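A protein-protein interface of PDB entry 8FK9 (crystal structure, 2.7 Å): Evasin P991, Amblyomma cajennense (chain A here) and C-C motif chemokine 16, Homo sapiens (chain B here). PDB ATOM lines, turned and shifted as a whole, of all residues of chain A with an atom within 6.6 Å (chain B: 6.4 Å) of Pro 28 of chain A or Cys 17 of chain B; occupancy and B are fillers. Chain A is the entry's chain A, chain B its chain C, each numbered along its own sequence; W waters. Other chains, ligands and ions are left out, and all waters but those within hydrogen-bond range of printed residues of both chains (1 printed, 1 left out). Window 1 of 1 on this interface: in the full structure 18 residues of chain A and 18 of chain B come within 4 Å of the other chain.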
ATOM      1  N   CYS A  25      30.233  -8.393  36.384  1.00  0.00           N
ATOM      2  CA  CYS A  25      29.989  -9.498  35.466  1.00  0.00           C
ATOM      3  C   CYS A  25      29.270  -9.043  34.203  1.00  0.00           C
ATOM      4  O   CYS A  25      28.549  -9.825  33.577  1.00  0.00           O
ATOM      5  CB  CYS A  25      29.198 -10.602  36.163  1.00  0.00           C
ATOM      6  SG  CYS A  25      30.168 -11.471  37.397  1.00  0.00           S
ATOM      7  N   THR A  26      29.469  -7.790  33.802  1.00  0.00           N
ATOM      8  CA  THR A  26      28.851  -7.247  32.602  1.00  0.00           C
ATOM      9  C   THR A  26      29.808  -7.241  31.417  1.00  0.00           C
ATOM     10  O   THR A  26      29.596  -6.493  30.456  1.00  0.00           O
ATOM     11  CB  THR A  26      28.331  -5.835  32.863  1.00  0.00           C
ATOM     12  OG1 THR A  26      29.366  -5.049  33.466  1.00  0.00           O
ATOM     13  CG2 THR A  26      27.124  -5.876  33.787  1.00  0.00           C
ATOM     14  N   CYS A  27      30.853  -8.046  31.469  1.00  0.00           N
ATOM     15  CA  CYS A  27      31.801  -8.119  30.375  1.00  0.00           C
ATOM     16  C   CYS A  27      31.465  -9.273  29.438  1.00  0.00           C
ATOM     17  O   CYS A  27      30.932 -10.302  29.869  1.00  0.00           O
ATOM     18  CB  CYS A  27      33.224  -8.305  30.908  1.00  0.00           C
ATOM     19  SG  CYS A  27      33.544  -9.965  31.553  1.00  0.00           S
ATOM     20  N   PRO A  28      31.750  -9.110  28.148  1.00  0.00           N
ATOM     21  CA  PRO A  28      31.563 -10.213  27.201  1.00  0.00           C
ATOM     22  C   PRO A  28      32.453 -11.395  27.554  1.00  0.00           C
ATOM     23  O   PRO A  28      33.464 -11.267  28.247  1.00  0.00           O
ATOM     24  CB  PRO A  28      31.970  -9.612  25.849  1.00  0.00           C
ATOM     25  CG  PRO A  28      32.088  -8.148  26.045  1.00  0.00           C
ATOM     26  CD  PRO A  28      31.982  -7.812  27.494  1.00  0.00           C
ATOM     27  N   ALA A  29      32.061 -12.566  27.062  1.00  0.00           N
ATOM     28  CA  ALA A  29      32.804 -13.793  27.288  1.00  0.00           C
ATOM     29  C   ALA A  29      33.086 -14.478  25.959  1.00  0.00           C
ATOM     30  O   ALA A  29      32.299 -14.357  25.016  1.00  0.00           O
ATOM     31  CB  ALA A  29      32.036 -14.757  28.199  1.00  0.00           C
ATOM     32  N   PRO A  30      34.201 -15.201  25.858  1.00  0.00           N
ATOM     33  CA  PRO A  30      34.507 -15.894  24.602  1.00  0.00           C
ATOM     34  C   PRO A  30      33.481 -16.981  24.312  1.00  0.00           C
ATOM     35  O   PRO A  30      33.087 -17.745  25.195  1.00  0.00           O
ATOM     36  CB  PRO A  30      35.901 -16.482  24.849  1.00  0.00           C
ATOM     37  CG  PRO A  30      36.465 -15.682  25.982  1.00  0.00           C
ATOM     38  CD  PRO A  30      35.290 -15.327  26.839  1.00  0.00           C
ATOM     39  N   HIS A  31      33.047 -17.033  23.056  1.00  0.00           N
ATOM     40  CA  HIS A  31      32.063 -17.998  22.595  1.00  0.00           C
ATOM     41  C   HIS A  31      32.560 -18.645  21.312  1.00  0.00           C
ATOM     42  O   HIS A  31      33.387 -18.085  20.589  1.00  0.00           O
ATOM     43  CB  HIS A  31      30.704 -17.338  22.344  1.00  0.00           C
ATOM     44  CG  HIS A  31      29.851 -17.224  23.567  1.00  0.00           C
ATOM     45  ND1 HIS A  31      30.180 -16.411  24.629  1.00  0.00           N
ATOM     46  CD2 HIS A  31      28.671 -17.802  23.887  1.00  0.00           C
ATOM     47  CE1 HIS A  31      29.246 -16.505  25.559  1.00  0.00           C
ATOM     48  NE2 HIS A  31      28.317 -17.343  25.132  1.00  0.00           N
ATOM     49  N   VAL A  39      22.691 -19.810  17.804  1.00  0.00           N
ATOM     50  CA  VAL A  39      23.444 -18.829  18.605  1.00  0.00           C
ATOM     51  C   VAL A  39      24.798 -19.405  19.015  1.00  0.00           C
ATOM     52  O   VAL A  39      25.004 -20.623  19.075  1.00  0.00           O
ATOM     53  CB  VAL A  39      22.661 -18.359  19.846  1.00  0.00           C
ATOM     54  CG1 VAL A  39      21.364 -17.665  19.464  1.00  0.00           C
ATOM     55  CG2 VAL A  39      22.408 -19.510  20.807  1.00  0.00           C
ATOM     56  N   MET A  40      25.735 -18.505  19.308  1.00  0.00           N
ATOM     57  CA  MET A  40      27.058 -18.917  19.762  1.00  0.00           C
ATOM     58  C   MET A  40      27.000 -19.415  21.203  1.00  0.00           C
ATOM     59  O   MET A  40      26.253 -18.887  22.031  1.00  0.00           O
ATOM     60  CB  MET A  40      28.053 -17.765  19.634  1.00  0.00           C
ATOM     61  CG  MET A  40      28.346 -17.373  18.192  1.00  0.00           C
ATOM     62  SD  MET A  40      29.477 -15.976  18.064  1.00  0.00           S
ATOM     63  CE  MET A  40      28.322 -14.616  17.886  1.00  0.00           C
ATOM     64  N   LYS A  41      27.791 -20.444  21.498  1.00  0.00           N
ATOM     65  CA  LYS A  41      27.749 -21.102  22.793  1.00  0.00           C
ATOM     66  C   LYS A  41      29.149 -21.211  23.383  1.00  0.00           C
ATOM     67  O   LYS A  41      30.114 -21.484  22.658  1.00  0.00           O
ATOM     68  CB  LYS A  41      27.113 -22.495  22.671  1.00  0.00           C
ATOM     69  CG  LYS A  41      25.716 -22.468  22.066  1.00  0.00           C
ATOM     70  CD  LYS A  41      25.185 -23.863  21.797  1.00  0.00           C
ATOM     71  CE  LYS A  41      23.854 -23.805  21.062  1.00  0.00           C
ATOM     72  NZ  LYS A  41      23.975 -23.130  19.739  1.00  0.00           N
ATOM     73  N   TYR A  47      32.843 -17.576  33.318  1.00  0.00           N
ATOM     74  CA  TYR A  47      33.629 -16.620  32.559  1.00  0.00           C
ATOM     75  C   TYR A  47      34.264 -15.617  33.509  1.00  0.00           C
ATOM     76  O   TYR A  47      33.786 -15.392  34.624  1.00  0.00           O
ATOM     77  CB  TYR A  47      32.790 -15.910  31.484  1.00  0.00           C
ATOM     78  CG  TYR A  47      31.630 -15.077  31.988  1.00  0.00           C
ATOM     79  CD1 TYR A  47      30.483 -15.675  32.494  1.00  0.00           C
ATOM     80  CD2 TYR A  47      31.666 -13.693  31.915  1.00  0.00           C
ATOM     81  CE1 TYR A  47      29.418 -14.915  32.939  1.00  0.00           C
ATOM     82  CE2 TYR A  47      30.605 -12.925  32.357  1.00  0.00           C
ATOM     83  CZ  TYR A  47      29.485 -13.541  32.866  1.00  0.00           C
ATOM     84  OH  TYR A  47      28.429 -12.778  33.307  1.00  0.00           O
ATOM     85  N   THR A  48      35.357 -15.022  33.046  1.00  0.00           N
ATOM     86  CA  THR A  48      36.173 -14.102  33.828  1.00  0.00           C
ATOM     87  C   THR A  48      36.097 -12.716  33.207  1.00  0.00           C
ATOM     88  O   THR A  48      36.217 -12.573  31.985  1.00  0.00           O
ATOM     89  CB  THR A  48      37.629 -14.568  33.893  1.00  0.00           C
ATOM     90  OG1 THR A  48      37.680 -15.933  34.324  1.00  0.00           O
ATOM     91  CG2 THR A  48      38.416 -13.708  34.870  1.00  0.00           C
ATOM     92  N   CYS A  49      35.886 -11.701  34.043  1.00  0.00           N
ATOM     93  CA  CYS A  49      35.914 -10.325  33.562  1.00  0.00           C
ATOM     94  C   CYS A  49      37.287  -9.708  33.803  1.00  0.00           C
ATOM     95  O   CYS A  49      38.107  -9.624  32.881  1.00  0.00           O
ATOM     96  CB  CYS A  49      34.821  -9.506  34.246  1.00  0.00           C
ATOM     97  SG  CYS A  49      33.183  -9.794  33.545  1.00  0.00           S
ATOM     98  N   TYR A  60      21.378 -21.255  30.533  1.00  0.00           N
ATOM     99  CA  TYR A  60      22.061 -20.673  29.388  1.00  0.00           C
ATOM    100  C   TYR A  60      22.706 -21.767  28.544  1.00  0.00           C
ATOM    101  O   TYR A  60      23.270 -22.723  29.096  1.00  0.00           O
ATOM    102  CB  TYR A  60      23.117 -19.675  29.873  1.00  0.00           C
ATOM    103  CG  TYR A  60      23.731 -18.785  28.812  1.00  0.00           C
ATOM    104  CD1 TYR A  60      24.873 -19.177  28.128  1.00  0.00           C
ATOM    105  CD2 TYR A  60      23.182 -17.544  28.515  1.00  0.00           C
ATOM    106  CE1 TYR A  60      25.447 -18.366  27.168  1.00  0.00           C
ATOM    107  CE2 TYR A  60      23.748 -16.724  27.559  1.00  0.00           C
ATOM    108  CZ  TYR A  60      24.880 -17.139  26.887  1.00  0.00           C
ATOM    109  OH  TYR A  60      25.442 -16.324  25.930  1.00  0.00           O
ATOM    110  N   PRO B  14      33.277  -9.787  17.994  1.00  0.00           N
ATOM    111  CA  PRO B  14      32.197 -10.523  17.333  1.00  0.00           C
ATOM    112  C   PRO B  14      32.153 -11.990  17.742  1.00  0.00           C
ATOM    113  O   PRO B  14      31.123 -12.647  17.566  1.00  0.00           O
ATOM    114  CB  PRO B  14      32.519 -10.380  15.843  1.00  0.00           C
ATOM    115  CG  PRO B  14      33.958  -9.925  15.765  1.00  0.00           C
ATOM    116  CD  PRO B  14      34.478  -9.686  17.154  1.00  0.00           C
ATOM    117  N   SER B  15      33.258 -12.508  18.275  1.00  0.00           N
ATOM    118  CA  SER B  15      33.299 -13.858  18.816  1.00  0.00           C
ATOM    119  C   SER B  15      32.962 -13.896  20.300  1.00  0.00           C
ATOM    120  O   SER B  15      33.267 -14.889  20.972  1.00  0.00           O
ATOM    121  CB  SER B  15      34.677 -14.485  18.581  1.00  0.00           C
ATOM    122  OG  SER B  15      35.666 -13.836  19.358  1.00  0.00           O
ATOM    123  N   THR B  16      32.353 -12.838  20.827  1.00  0.00           N
ATOM    124  CA  THR B  16      32.001 -12.758  22.234  1.00  0.00           C
ATOM    125  C   THR B  16      30.503 -12.539  22.389  1.00  0.00           C
ATOM    126  O   THR B  16      29.862 -11.895  21.555  1.00  0.00           O
ATOM    127  CB  THR B  16      32.753 -11.617  22.934  1.00  0.00           C
ATOM    128  OG1 THR B  16      32.360 -10.364  22.361  1.00  0.00           O
ATOM    129  CG2 THR B  16      34.256 -11.789  22.776  1.00  0.00           C
ATOM    130  N   CYS B  17      29.954 -13.071  23.478  1.00  0.00           N
ATOM    131  CA  CYS B  17      28.550 -12.900  23.815  1.00  0.00           C
ATOM    132  C   CYS B  17      28.440 -12.445  25.263  1.00  0.00           C
ATOM    133  O   CYS B  17      29.363 -12.617  26.064  1.00  0.00           O
ATOM    134  CB  CYS B  17      27.745 -14.189  23.599  1.00  0.00           C
ATOM    135  SG  CYS B  17      27.468 -14.623  21.863  1.00  0.00           S
ATOM    136  N   CYS B  18      27.296 -11.856  25.592  1.00  0.00           N
ATOM    137  CA  CYS B  18      27.062 -11.285  26.910  1.00  0.00           C
ATOM    138  C   CYS B  18      26.118 -12.161  27.717  1.00  0.00           C
ATOM    139  O   CYS B  18      25.143 -12.700  27.187  1.00  0.00           O
ATOM    140  CB  CYS B  18      26.497  -9.874  26.794  1.00  0.00           C
ATOM    141  SG  CYS B  18      27.713  -8.707  26.177  1.00  0.00           S
ATOM    142  N   LEU B  19      26.409 -12.284  29.010  1.00  0.00           N
ATOM    143  CA  LEU B  19      25.637 -13.123  29.905  1.00  0.00           C
ATOM    144  C   LEU B  19      24.907 -12.337  30.981  1.00  0.00           C
ATOM    145  O   LEU B  19      24.031 -12.900  31.646  1.00  0.00           O
ATOM    146  CB  LEU B  19      26.544 -14.176  30.559  1.00  0.00           C
ATOM    147  CG  LEU B  19      27.379 -14.943  29.532  1.00  0.00           C
ATOM    148  CD1 LEU B  19      28.801 -14.421  29.499  1.00  0.00           C
ATOM    149  CD2 LEU B  19      27.357 -16.428  29.815  1.00  0.00           C
ATOM    150  N   ALA B  37      26.818  -7.627  19.422  1.00  0.00           N
ATOM    151  CA  ALA B  37      26.893  -9.076  19.634  1.00  0.00           C
ATOM    152  C   ALA B  37      25.459  -9.600  19.639  1.00  0.00           C
ATOM    153  O   ALA B  37      24.858  -9.800  20.700  1.00  0.00           O
ATOM    154  CB  ALA B  37      27.635  -9.410  20.927  1.00  0.00           C
ATOM    155  N   ASN B  39      24.163 -12.350  17.445  1.00  0.00           N
ATOM    156  CA  ASN B  39      23.962 -13.783  17.259  1.00  0.00           C
ATOM    157  C   ASN B  39      24.226 -14.522  18.565  1.00  0.00           C
ATOM    158  O   ASN B  39      24.978 -15.500  18.598  1.00  0.00           O
ATOM    159  CB  ASN B  39      24.861 -14.321  16.145  1.00  0.00           C
ATOM    160  CG  ASN B  39      24.358 -15.638  15.577  1.00  0.00           C
ATOM    161  OD1 ASN B  39      23.374 -15.676  14.835  1.00  0.00           O
ATOM    162  ND2 ASN B  39      25.031 -16.727  15.931  1.00  0.00           N
ATOM    163  N   CYS B  40      23.601 -14.057  19.642  1.00  0.00           N
ATOM    164  CA  CYS B  40      23.799 -14.602  20.974  1.00  0.00           C
ATOM    165  C   CYS B  40      22.447 -14.864  21.617  1.00  0.00           C
ATOM    166  O   CYS B  40      21.428 -14.294  21.218  1.00  0.00           O
ATOM    167  CB  CYS B  40      24.615 -13.650  21.860  1.00  0.00           C
ATOM    168  SG  CYS B  40      26.216 -13.178  21.184  1.00  0.00           S
ATOM    169  N   HIS B  41      22.451 -15.746  22.619  1.00  0.00           N
ATOM    170  CA  HIS B  41      21.231 -16.002  23.375  1.00  0.00           C
ATOM    171  C   HIS B  41      20.743 -14.731  24.055  1.00  0.00           C
ATOM    172  O   HIS B  41      19.534 -14.493  24.156  1.00  0.00           O
ATOM    173  CB  HIS B  41      21.477 -17.103  24.405  1.00  0.00           C
ATOM    174  CG  HIS B  41      20.289 -17.402  25.265  1.00  0.00           C
ATOM    175  ND1 HIS B  41      19.126 -17.946  24.765  1.00  0.00           N
ATOM    176  CD2 HIS B  41      20.084 -17.230  26.592  1.00  0.00           C
ATOM    177  CE1 HIS B  41      18.256 -18.098  25.746  1.00  0.00           C
ATOM    178  NE2 HIS B  41      18.811 -17.671  26.866  1.00  0.00           N
ATOM    179  N   LEU B  42      21.674 -13.894  24.515  1.00  0.00           N
ATOM    180  CA  LEU B  42      21.368 -12.562  25.026  1.00  0.00           C
ATOM    181  C   LEU B  42      21.983 -11.539  24.081  1.00  0.00           C
ATOM    182  O   LEU B  42      23.131 -11.115  24.278  1.00  0.00           O
ATOM    183  CB  LEU B  42      21.901 -12.377  26.450  1.00  0.00           C
ATOM    184  CG  LEU B  42      21.324 -13.324  27.504  1.00  0.00           C
ATOM    185  CD1 LEU B  42      22.189 -13.333  28.759  1.00  0.00           C
ATOM    186  CD2 LEU B  42      19.885 -12.946  27.839  1.00  0.00           C
ATOM    187  N   ALA B  44      23.332  -8.294  22.621  1.00  0.00           N
ATOM    188  CA  ALA B  44      23.808  -7.183  23.426  1.00  0.00           C
ATOM    189  C   ALA B  44      24.550  -6.179  22.561  1.00  0.00           C
ATOM    190  O   ALA B  44      25.163  -6.535  21.551  1.00  0.00           O
ATOM    191  CB  ALA B  44      24.729  -7.665  24.556  1.00  0.00           C
ATOM    192  N   ILE B  46      27.687  -3.786  23.052  1.00  0.00           N
ATOM    193  CA  ILE B  46      28.850  -3.753  23.933  1.00  0.00           C
ATOM    194  C   ILE B  46      29.497  -2.381  23.809  1.00  0.00           C
ATOM    195  O   ILE B  46      30.099  -2.061  22.780  1.00  0.00           O
ATOM    196  CB  ILE B  46      29.846  -4.865  23.582  1.00  0.00           C
ATOM    197  CG1 ILE B  46      29.208  -6.234  23.811  1.00  0.00           C
ATOM    198  CG2 ILE B  46      31.123  -4.715  24.407  1.00  0.00           C
ATOM    199  CD1 ILE B  46      30.028  -7.384  23.282  1.00  0.00           C
ATOM    200  N   GLU B  54      34.710  -3.391  28.403  1.00  0.00           N
ATOM    201  CA  GLU B  54      33.590  -3.768  27.558  1.00  0.00           C
ATOM    202  C   GLU B  54      32.389  -4.024  28.462  1.00  0.00           C
ATOM    203  O   GLU B  54      32.455  -4.860  29.369  1.00  0.00           O
ATOM    204  CB  GLU B  54      33.940  -4.995  26.719  1.00  0.00           C
ATOM    205  CG  GLU B  54      34.941  -4.693  25.610  1.00  0.00           C
ATOM    206  CD  GLU B  54      35.125  -5.849  24.646  1.00  0.00           C
ATOM    207  OE1 GLU B  54      34.112  -6.345  24.113  1.00  0.00           O
ATOM    208  OE2 GLU B  54      36.284  -6.258  24.417  1.00  0.00           O
ATOM    209  N   VAL B  55      31.308  -3.285  28.225  1.00  0.00           N
ATOM    210  CA  VAL B  55      30.141  -3.271  29.101  1.00  0.00           C
ATOM    211  C   VAL B  55      28.936  -3.730  28.293  1.00  0.00           C
ATOM    212  O   VAL B  55      28.585  -3.109  27.282  1.00  0.00           O
ATOM    213  CB  VAL B  55      29.897  -1.882  29.711  1.00  0.00           C
ATOM    214  CG1 VAL B  55      28.837  -1.962  30.795  1.00  0.00           C
ATOM    215  CG2 VAL B  55      31.193  -1.310  30.274  1.00  0.00           C
ATOM    216  N   CYS B  56      28.294  -4.798  28.752  1.00  0.00           N
ATOM    217  CA  CYS B  56      27.163  -5.378  28.042  1.00  0.00           C
ATOM    218  C   CYS B  56      25.878  -4.641  28.385  1.00  0.00           C
ATOM    219  O   CYS B  56      25.570  -4.430  29.561  1.00  0.00           O
ATOM    220  CB  CYS B  56      27.029  -6.853  28.402  1.00  0.00           C
ATOM    221  SG  CYS B  56      28.418  -7.845  27.868  1.00  0.00           S
HETATM  222  O   HOH W   1      31.669  -4.644  32.164  1.00  0.00           O
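Of the 14 printed residues of chain A, 10 touch a printed residue of chain B.
Printed residues of chain A that touch a printed residue of chain B: Thr 26, Cys 27, Pro 28, Ala 29, Pro 30, His 31, Val 39, Met 40, Tyr 47 and Tyr 60.
Hydrophobic or aromatic side chains of chain A that line the printed part of chain B: Pro 28, Ala 29, His 31, Val 39, Met 40, Tyr 47 and Tyr 60.
Hydrophobic or aromatic side chains of chain B that line the printed part of chain A: Leu 19, His 41, Leu 42 and Ile 46.
Along chain B the printed residues that touch a printed residue of chain A span positions 14 to 56.
Among the printed residues, no Asp or Glu carboxylate lies within 4 Å of a Lys or Arg side-chain nitrogen of the other chain.
Of chain B, only Thr 16 (3.6 Å), Cys 17 (3.5 Å), Ile 46 (3.5 Å), Glu 54 (3.3 Å) and Cys 56 (3.6 Å) come within 4 Å of Pro 28 of chain A.
Lys 41 of chain A touches none of the printed residues of chain B.
Cys 49 of chain A touches none of the printed residues of chain B.
Of the printed residues of chain A, Pro 14 of chain B touches Met 40 (3.4 Å).
Cys 17 of chain B touches just these residues of chain A: Pro 28, Ala 29, His 31, Met 40 and Tyr 60.
Of the printed residues of chain A, His 41 of chain B touches Val 39 and Tyr 60.
The nearest residue of chain B that does not touch Pro 28 of chain A is Cys 18 of chain B (4.3 Å).
The nearest residue of chain A that does not touch Cys 17 of chain B is Cys 27 of chain A (4.7 Å).
Among the printed residues, pairs that only touch across the chains: Thr 26 of chain A with Val 55 of chain B, Cys 27 of chain A with Glu 54 of chain B, Cys 27 of chain A with Cys 56 of chain B, Pro 28 of chain A with Thr 16 of chain B, Pro 28 of chain A with Cys 17 of chain B, Pro 28 of chain A with Ile 46 of chain B, Pro 28 of chain A with Glu 54 of chain B, Ala 29 of chain A with Thr 16 of chain B, Ala 29 of chain A with Leu 19 of chain B, Pro 30 of chain A with Ser 15 of chain B, His 31 of chain A with Cys 17 of chain B, Val 39 of chain A with Asn 39 of chain B, Val 39 of chain A with Cys 40 of chain B, Val 39 of chain A with His 41 of chain B, Met 40 of chain A with Cys 17 of chain B, Tyr 47 of chain A with Leu 19 of chain B, Tyr 60 of chain A with Cys 17 of chain B, Tyr 60 of chain A with Cys 18 of chain B, Tyr 60 of chain A with Leu 19 of chain B, Tyr 60 of chain A with His 41 of chain B and Tyr 60 of chain A with Leu 42 of chain B.
Water W1 bridges the side-chain hydroxyl of Thr 26 of chain A (2.7 Å) and the backbone carbonyl oxygen of Glu 54 of chain B (2.9 Å).
O of Asn 39 of chain B sits at hydrogen-bond distance from N of Met 40 of chain A.
The backbone NH (N) of Ala 29 of chain A is in hydrogen-bond range of the backbone carbonyl oxygen (O) of Cys 17 of chain B (2.9 Å).
O of Thr 26 of chain A lies close to O of Glu 54 of chain B.
The backbone nitrogen (N) of Pro 28 of chain A sits close to the side-chain sulfur (SG) of Cys 56 of chain B, at 3.6 Å.
N of Cys 56 of chain B is in hydrogen-bond range of O of Thr 26 of chain A, at 2.7 Å.
SD of Met 40 of chain A sits close to O of Pro 14 of chain B (3.7 Å).
The backbone NH (N) of His 31 of chain A lies within hydrogen-bond range of the backbone carbonyl oxygen (O) of Ser 15 of chain B.
ND1 of His 31 of chain A lies within hydrogen-bond range of O of Ala 29 of chain A, at 3.0 Å.
The side-chain sulfur of Cys 56 of chain B is disulfide-bonded to the side-chain sulfur of Cys 18 of chain B (2.0 Å).
SG of Cys 17 of chain B forms a disulfide with SG of Cys 40 of chain B (2.0 Å).
O of Cys 25 of chain A sits at hydrogen-bond distance from OH of Tyr 47 of chain A (3.0 Å).
A ring nitrogen (NE2) of His 31 of chain A lies within hydrogen-bond range of the side-chain hydroxyl of Tyr 60 of chain A (3.2 Å).
O of Val 39 of chain A lies within hydrogen-bond range of NZ of Lys 41 of chain A, 2.8 Å away.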
